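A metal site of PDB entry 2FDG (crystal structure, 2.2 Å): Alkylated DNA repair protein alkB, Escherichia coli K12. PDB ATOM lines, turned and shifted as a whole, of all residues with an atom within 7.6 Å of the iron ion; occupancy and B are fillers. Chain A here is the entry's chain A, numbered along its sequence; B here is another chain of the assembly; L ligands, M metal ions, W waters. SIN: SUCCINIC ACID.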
ATOM      1  N   MET A  51       6.994 -18.056  13.713  1.00  0.00           N
ATOM      2  CA  MET A  51       6.486 -16.844  13.083  1.00  0.00           C
ATOM      3  C   MET A  51       5.013 -16.837  12.720  1.00  0.00           C
ATOM      4  O   MET A  51       4.340 -17.868  12.727  1.00  0.00           O
ATOM      5  CB  MET A  51       7.288 -16.549  11.798  1.00  0.00           C
ATOM      6  CG  MET A  51       8.736 -16.119  11.988  1.00  0.00           C
ATOM      7  SD  MET A  51       9.642 -16.181  10.438  1.00  0.00           S
ATOM      8  CE  MET A  51      11.066 -15.183  10.829  1.00  0.00           C
ATOM      9  N   LEU A 108       5.711  -8.798  10.484  1.00  0.00           N
ATOM     10  CA  LEU A 108       6.167 -10.149  10.784  1.00  0.00           C
ATOM     11  C   LEU A 108       6.423 -10.247  12.281  1.00  0.00           C
ATOM     12  O   LEU A 108       7.172  -9.445  12.844  1.00  0.00           O
ATOM     13  CB  LEU A 108       7.447 -10.471   9.984  1.00  0.00           C
ATOM     14  CG  LEU A 108       8.155 -11.829  10.123  1.00  0.00           C
ATOM     15  CD1 LEU A 108       7.231 -13.006   9.753  1.00  0.00           C
ATOM     16  CD2 LEU A 108       9.403 -11.831   9.266  1.00  0.00           C
ATOM     17  N   ASN A 110       7.863 -12.461  15.222  1.00  0.00           N
ATOM     18  CA  ASN A 110       8.790 -13.530  15.559  1.00  0.00           C
ATOM     19  C   ASN A 110       8.679 -13.884  17.039  1.00  0.00           C
ATOM     20  O   ASN A 110       8.644 -12.986  17.877  1.00  0.00           O
ATOM     21  CB  ASN A 110      10.236 -13.078  15.284  1.00  0.00           C
ATOM     22  CG  ASN A 110      10.585 -12.970  13.803  1.00  0.00           C
ATOM     23  OD1 ASN A 110      11.753 -12.825  13.451  1.00  0.00           O
ATOM     24  ND2 ASN A 110       9.580 -13.028  12.933  1.00  0.00           N
ATOM     25  N   TYR A 112      10.583 -16.057  19.990  1.00  0.00           N
ATOM     26  CA  TYR A 112      11.831 -16.728  20.348  1.00  0.00           C
ATOM     27  C   TYR A 112      11.715 -17.503  21.640  1.00  0.00           C
ATOM     28  O   TYR A 112      11.547 -16.925  22.703  1.00  0.00           O
ATOM     29  CB  TYR A 112      12.971 -15.715  20.511  1.00  0.00           C
ATOM     30  CG  TYR A 112      13.299 -14.945  19.255  1.00  0.00           C
ATOM     31  CD1 TYR A 112      12.539 -13.810  18.889  1.00  0.00           C
ATOM     32  CD2 TYR A 112      14.346 -15.347  18.415  1.00  0.00           C
ATOM     33  CE1 TYR A 112      12.830 -13.094  17.710  1.00  0.00           C
ATOM     34  CE2 TYR A 112      14.638 -14.639  17.221  1.00  0.00           C
ATOM     35  CZ  TYR A 112      13.885 -13.517  16.874  1.00  0.00           C
ATOM     36  OH  TYR A 112      14.144 -12.837  15.712  1.00  0.00           O
ATOM     37  N   LEU A 118      18.471 -17.141  14.838  1.00  0.00           N
ATOM     38  CA  LEU A 118      18.234 -16.744  13.462  1.00  0.00           C
ATOM     39  C   LEU A 118      19.614 -16.416  12.907  1.00  0.00           C
ATOM     40  O   LEU A 118      20.303 -15.518  13.410  1.00  0.00           O
ATOM     41  CB  LEU A 118      17.307 -15.519  13.441  1.00  0.00           C
ATOM     42  CG  LEU A 118      16.461 -15.153  12.228  1.00  0.00           C
ATOM     43  CD1 LEU A 118      15.691 -16.346  11.675  1.00  0.00           C
ATOM     44  CD2 LEU A 118      15.512 -14.042  12.640  1.00  0.00           C
ATOM     45  N   SER A 119      20.052 -17.202  11.923  1.00  0.00           N
ATOM     46  CA  SER A 119      21.370 -17.018  11.294  1.00  0.00           C
ATOM     47  C   SER A 119      21.378 -15.822  10.345  1.00  0.00           C
ATOM     48  O   SER A 119      20.321 -15.334   9.951  1.00  0.00           O
ATOM     49  CB  SER A 119      21.804 -18.291  10.566  1.00  0.00           C
ATOM     50  OG  SER A 119      20.887 -18.646   9.548  1.00  0.00           O
ATOM     51  N   HIS A 121      21.305 -13.130   7.584  1.00  0.00           N
ATOM     52  CA  HIS A 121      20.500 -12.933   6.376  1.00  0.00           C
ATOM     53  C   HIS A 121      20.218 -11.448   6.142  1.00  0.00           C
ATOM     54  O   HIS A 121      20.416 -10.616   7.029  1.00  0.00           O
ATOM     55  CB  HIS A 121      19.149 -13.674   6.487  1.00  0.00           C
ATOM     56  CG  HIS A 121      18.242 -13.124   7.554  1.00  0.00           C
ATOM     57  ND1 HIS A 121      18.433 -13.372   8.890  1.00  0.00           N
ATOM     58  CD2 HIS A 121      17.198 -12.255   7.486  1.00  0.00           C
ATOM     59  CE1 HIS A 121      17.549 -12.689   9.604  1.00  0.00           C
ATOM     60  NE2 HIS A 121      16.787 -12.006   8.774  1.00  0.00           N
ATOM     61  N   GLN A 122      19.642 -11.175   4.982  1.00  0.00           N
ATOM     62  CA  GLN A 122      19.232  -9.835   4.599  1.00  0.00           C
ATOM     63  C   GLN A 122      17.725  -9.895   4.378  1.00  0.00           C
ATOM     64  O   GLN A 122      17.185 -10.955   4.045  1.00  0.00           O
ATOM     65  CB  GLN A 122      19.876  -9.393   3.286  1.00  0.00           C
ATOM     66  CG  GLN A 122      21.315  -8.961   3.390  1.00  0.00           C
ATOM     67  CD  GLN A 122      21.901  -8.575   2.050  1.00  0.00           C
ATOM     68  OE1 GLN A 122      21.865  -9.359   1.097  1.00  0.00           O
ATOM     69  NE2 GLN A 122      22.473  -7.389   1.982  1.00  0.00           N
ATOM     70  N   ASP A 123      17.069  -8.763   4.624  1.00  0.00           N
ATOM     71  CA  ASP A 123      15.643  -8.613   4.398  1.00  0.00           C
ATOM     72  C   ASP A 123      15.556  -7.865   3.080  1.00  0.00           C
ATOM     73  O   ASP A 123      15.688  -6.630   3.035  1.00  0.00           O
ATOM     74  CB  ASP A 123      15.006  -7.822   5.542  1.00  0.00           C
ATOM     75  CG  ASP A 123      14.647  -8.692   6.723  1.00  0.00           C
ATOM     76  OD1 ASP A 123      15.556  -9.082   7.485  1.00  0.00           O
ATOM     77  OD2 ASP A 123      13.452  -9.004   6.886  1.00  0.00           O
ATOM     78  N   LYS A 124      15.400  -8.624   1.996  1.00  0.00           N
ATOM     79  CA  LYS A 124      15.337  -8.060   0.644  1.00  0.00           C
ATOM     80  C   LYS A 124      14.201  -8.573  -0.256  1.00  0.00           C
ATOM     81  O   LYS A 124      14.359  -8.723  -1.468  1.00  0.00           O
ATOM     82  CB  LYS A 124      16.721  -8.219  -0.045  1.00  0.00           C
ATOM     83  CG  LYS A 124      17.265  -9.648  -0.056  1.00  0.00           C
ATOM     84  CD  LYS A 124      18.652  -9.711  -0.683  1.00  0.00           C
ATOM     85  CE  LYS A 124      19.132 -11.157  -0.800  1.00  0.00           C
ATOM     86  NZ  LYS A 124      20.497 -11.236  -1.362  1.00  0.00           N
ATOM     87  N   ILE A 133      12.514  -0.451   8.077  1.00  0.00           N
ATOM     88  CA  ILE A 133      11.838  -1.545   8.766  1.00  0.00           C
ATOM     89  C   ILE A 133      11.838  -1.109  10.233  1.00  0.00           C
ATOM     90  O   ILE A 133      12.871  -0.726  10.776  1.00  0.00           O
ATOM     91  CB  ILE A 133      12.569  -2.933   8.578  1.00  0.00           C
ATOM     92  CG1 ILE A 133      12.279  -3.499   7.178  1.00  0.00           C
ATOM     93  CG2 ILE A 133      12.102  -3.946   9.656  1.00  0.00           C
ATOM     94  CD1 ILE A 133      12.890  -4.866   6.880  1.00  0.00           C
ATOM     95  N   PHE A 144      21.297  -8.980  19.046  1.00  0.00           N
ATOM     96  CA  PHE A 144      21.145  -8.748  17.624  1.00  0.00           C
ATOM     97  C   PHE A 144      22.555  -8.567  17.056  1.00  0.00           C
ATOM     98  O   PHE A 144      23.267  -7.639  17.441  1.00  0.00           O
ATOM     99  CB  PHE A 144      20.308  -7.467  17.405  1.00  0.00           C
ATOM    100  CG  PHE A 144      19.971  -7.182  15.969  1.00  0.00           C
ATOM    101  CD1 PHE A 144      18.776  -7.667  15.415  1.00  0.00           C
ATOM    102  CD2 PHE A 144      20.834  -6.412  15.159  1.00  0.00           C
ATOM    103  CE1 PHE A 144      18.439  -7.404  14.074  1.00  0.00           C
ATOM    104  CE2 PHE A 144      20.516  -6.137  13.821  1.00  0.00           C
ATOM    105  CZ  PHE A 144      19.310  -6.631  13.270  1.00  0.00           C
ATOM    106  N   PHE A 175      21.900  -4.422   5.889  1.00  0.00           N
ATOM    107  CA  PHE A 175      22.898  -5.170   6.664  1.00  0.00           C
ATOM    108  C   PHE A 175      22.533  -6.636   6.844  1.00  0.00           C
ATOM    109  O   PHE A 175      21.361  -6.966   7.044  1.00  0.00           O
ATOM    110  CB  PHE A 175      23.078  -4.582   8.078  1.00  0.00           C
ATOM    111  CG  PHE A 175      23.977  -3.365   8.160  1.00  0.00           C
ATOM    112  CD1 PHE A 175      24.119  -2.699   9.395  1.00  0.00           C
ATOM    113  CD2 PHE A 175      24.669  -2.851   7.034  1.00  0.00           C
ATOM    114  CE1 PHE A 175      24.948  -1.540   9.527  1.00  0.00           C
ATOM    115  CE2 PHE A 175      25.495  -1.699   7.137  1.00  0.00           C
ATOM    116  CZ  PHE A 175      25.630  -1.041   8.389  1.00  0.00           C
ATOM    117  N   TYR A 176      23.551  -7.502   6.772  1.00  0.00           N
ATOM    118  CA  TYR A 176      23.376  -8.937   7.034  1.00  0.00           C
ATOM    119  C   TYR A 176      23.197  -8.993   8.551  1.00  0.00           C
ATOM    120  O   TYR A 176      23.947  -8.338   9.281  1.00  0.00           O
ATOM    121  CB  TYR A 176      24.619  -9.724   6.618  1.00  0.00           C
ATOM    122  CG  TYR A 176      24.541 -10.298   5.217  1.00  0.00           C
ATOM    123  CD1 TYR A 176      23.956 -11.555   4.982  1.00  0.00           C
ATOM    124  CD2 TYR A 176      25.078  -9.597   4.108  1.00  0.00           C
ATOM    125  CE1 TYR A 176      23.893 -12.115   3.666  1.00  0.00           C
ATOM    126  CE2 TYR A 176      25.020 -10.141   2.791  1.00  0.00           C
ATOM    127  CZ  TYR A 176      24.428 -11.398   2.589  1.00  0.00           C
ATOM    128  OH  TYR A 176      24.353 -11.930   1.329  1.00  0.00           O
ATOM    129  N   HIS A 177      22.165  -9.702   9.000  1.00  0.00           N
ATOM    130  CA  HIS A 177      21.862  -9.757  10.431  1.00  0.00           C
ATOM    131  C   HIS A 177      21.233 -11.044  10.936  1.00  0.00           C
ATOM    132  O   HIS A 177      20.688 -11.838  10.175  1.00  0.00           O
ATOM    133  CB  HIS A 177      20.969  -8.577  10.805  1.00  0.00           C
ATOM    134  CG  HIS A 177      19.667  -8.542  10.062  1.00  0.00           C
ATOM    135  ND1 HIS A 177      19.589  -8.186   8.731  1.00  0.00           N
ATOM    136  CD2 HIS A 177      18.414  -8.870  10.443  1.00  0.00           C
ATOM    137  CE1 HIS A 177      18.342  -8.314   8.322  1.00  0.00           C
ATOM    138  NE2 HIS A 177      17.604  -8.723   9.338  1.00  0.00           N
ATOM    139  N   GLY A 178      21.215 -11.169  12.260  1.00  0.00           N
ATOM    140  CA  GLY A 178      20.640 -12.334  12.908  1.00  0.00           C
ATOM    141  C   GLY A 178      20.511 -12.169  14.400  1.00  0.00           C
ATOM    142  O   GLY A 178      20.813 -11.109  14.957  1.00  0.00           O
ATOM    143  N   ASN A 196       9.137 -10.213  18.590  1.00  0.00           N
ATOM    144  CA  ASN A 196       9.684  -9.146  17.762  1.00  0.00           C
ATOM    145  C   ASN A 196       8.787  -8.882  16.585  1.00  0.00           C
ATOM    146  O   ASN A 196       8.491  -9.775  15.793  1.00  0.00           O
ATOM    147  CB  ASN A 196      11.106  -9.413  17.274  1.00  0.00           C
ATOM    148  CG  ASN A 196      11.678  -8.229  16.479  1.00  0.00           C
ATOM    149  OD1 ASN A 196      11.586  -8.198  15.255  1.00  0.00           O
ATOM    150  ND2 ASN A 196      12.213  -7.233  17.182  1.00  0.00           N
ATOM    151  N   THR A 198       8.296  -6.690  13.142  1.00  0.00           N
ATOM    152  CA  THR A 198       9.038  -5.951  12.125  1.00  0.00           C
ATOM    153  C   THR A 198       8.033  -5.475  11.091  1.00  0.00           C
ATOM    154  O   THR A 198       7.444  -6.280  10.365  1.00  0.00           O
ATOM    155  CB  THR A 198      10.205  -6.760  11.488  1.00  0.00           C
ATOM    156  OG1 THR A 198       9.811  -8.106  11.227  1.00  0.00           O
ATOM    157  CG2 THR A 198      11.447  -6.719  12.364  1.00  0.00           C
ATOM    158  N   ARG A 200       6.840  -3.662   7.801  1.00  0.00           N
ATOM    159  CA  ARG A 200       7.381  -3.508   6.446  1.00  0.00           C
ATOM    160  C   ARG A 200       6.402  -2.935   5.437  1.00  0.00           C
ATOM    161  O   ARG A 200       5.184  -3.119   5.559  1.00  0.00           O
ATOM    162  CB  ARG A 200       7.865  -4.863   5.900  1.00  0.00           C
ATOM    163  CG  ARG A 200       8.926  -5.589   6.701  1.00  0.00           C
ATOM    164  CD  ARG A 200       8.390  -6.884   7.288  1.00  0.00           C
ATOM    165  NE  ARG A 200       9.345  -7.499   8.208  1.00  0.00           N
ATOM    166  CZ  ARG A 200      10.428  -8.198   7.853  1.00  0.00           C
ATOM    167  NH1 ARG A 200      10.716  -8.395   6.576  1.00  0.00           N
ATOM    168  NH2 ARG A 200      11.251  -8.647   8.789  1.00  0.00           N
ATOM    169  C2  MA7 B   2      13.021 -13.522   7.805  1.00  0.00           C
ATOM    170  C4  MA7 B   2      14.684 -14.689   6.956  1.00  0.00           C
ATOM    171  C5  MA7 B   2      14.744 -13.891   5.831  1.00  0.00           C
ATOM    172  C6  MA7 B   2      13.837 -12.832   5.747  1.00  0.00           C
ATOM    173  C8  MA7 B   2      16.252 -15.373   5.594  1.00  0.00           C
ATOM    174  P   MA7 B   2      19.084 -17.877   4.560  1.00  0.00           P
ATOM    175  OP1 MA7 B   2      18.119 -17.568   3.473  1.00  0.00           O
ATOM    176  OP2 MA7 B   2      20.514 -17.508   4.391  1.00  0.00           O
ATOM    177  O5' MA7 B   2      18.546 -17.239   5.906  1.00  0.00           O
ATOM    178  N9  MA7 B   2      15.671 -15.630   6.810  1.00  0.00           N
ATOM    179  N3  MA7 B   2      13.834 -14.556   7.994  1.00  0.00           N
ATOM    180  N1  MA7 B   2      12.971 -12.671   6.768  1.00  0.00           N
ATOM    181  N6  MA7 B   2      13.771 -11.981   4.715  1.00  0.00           N
ATOM    182  N7  MA7 B   2      15.736 -14.336   4.970  1.00  0.00           N
ATOM    183  CN  MA7 B   2      11.963 -11.570   6.747  1.00  0.00           C
ATOM    184  C2' MA7 B   2      16.038 -18.081   7.206  1.00  0.00           C
ATOM    185  C5' MA7 B   2      19.180 -17.507   7.152  1.00  0.00           C
ATOM    186  C4' MA7 B   2      18.136 -17.620   8.237  1.00  0.00           C
ATOM    187  O4' MA7 B   2      17.357 -16.394   8.206  1.00  0.00           O
ATOM    188  C1' MA7 B   2      16.028 -16.666   7.775  1.00  0.00           C
ATOM    189  C3' MA7 B   2      17.132 -18.750   8.013  1.00  0.00           C
ATOM    190  O3' MA7 B   2      16.613 -19.173   9.279  1.00  0.00           O
HETATM  191  C1  SIN L   1      14.873  -9.258  15.697  1.00  0.00           C
HETATM  192  O1  SIN L   1      14.412 -10.255  16.202  1.00  0.00           O
HETATM  193  O2  SIN L   1      15.355  -8.288  16.461  1.00  0.00           O
HETATM  194  C2  SIN L   1      14.654  -8.992  14.252  1.00  0.00           C
HETATM  195  C3  SIN L   1      15.021 -10.212  13.427  1.00  0.00           C
HETATM  196  C4  SIN L   1      15.235  -9.824  11.982  1.00  0.00           C
HETATM  197  O3  SIN L   1      14.668  -8.854  11.506  1.00  0.00           O
HETATM  198  O4  SIN L   1      15.862 -10.675  11.174  1.00  0.00           O
HETATM  199 FE    FE M   1      15.845 -10.032   9.297  1.00  0.00          FE
HETATM  200  O   HOH W   1      14.887  -6.915   9.300  1.00  0.00           O
HETATM  201  O   HOH W   2      13.929 -10.827   9.067  1.00  0.00           O
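ND1 of His 121 is in hydrogen-bond range of O4' of MA7 2 of chain B (3.3 Å). ND1 of His 121 lies within hydrogen-bond range of O of Ser 119 (2.9 Å). The side-chain carboxylate (OD2) of Asp 123 is in salt-bridge range of the guanidinium group (NH1) of Arg 200 (2.8 Å). A ring nitrogen (ND1) of His 177 lies within hydrogen-bond range of the backbone carbonyl oxygen (O) of Phe 175 (2.7 Å).
Within 4 Å of the iron ion: His 121, Asp 123 and His 177. The nearest printed residue that does not touch the iron ion is MA7 2 of chain B (4.6 Å).
The iron ion is bound by an oxygen (O4) of the ligand, the side-chain carboxylate (OD1) of Asp 123, water W2, a ring nitrogen (NE2) of His 177 and a ring nitrogen (NE2) of His 121. Slightly farther from the iron ion lies O3 of the ligand (2.8 Å).
Water W2 lies within hydrogen-bond range of the side-chain carboxylate of Asp 123 (2.9 Å), N1 of MA7 2 of chain B (3.1 Å) and the guanidinium group of Arg 200 (3.5 Å).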
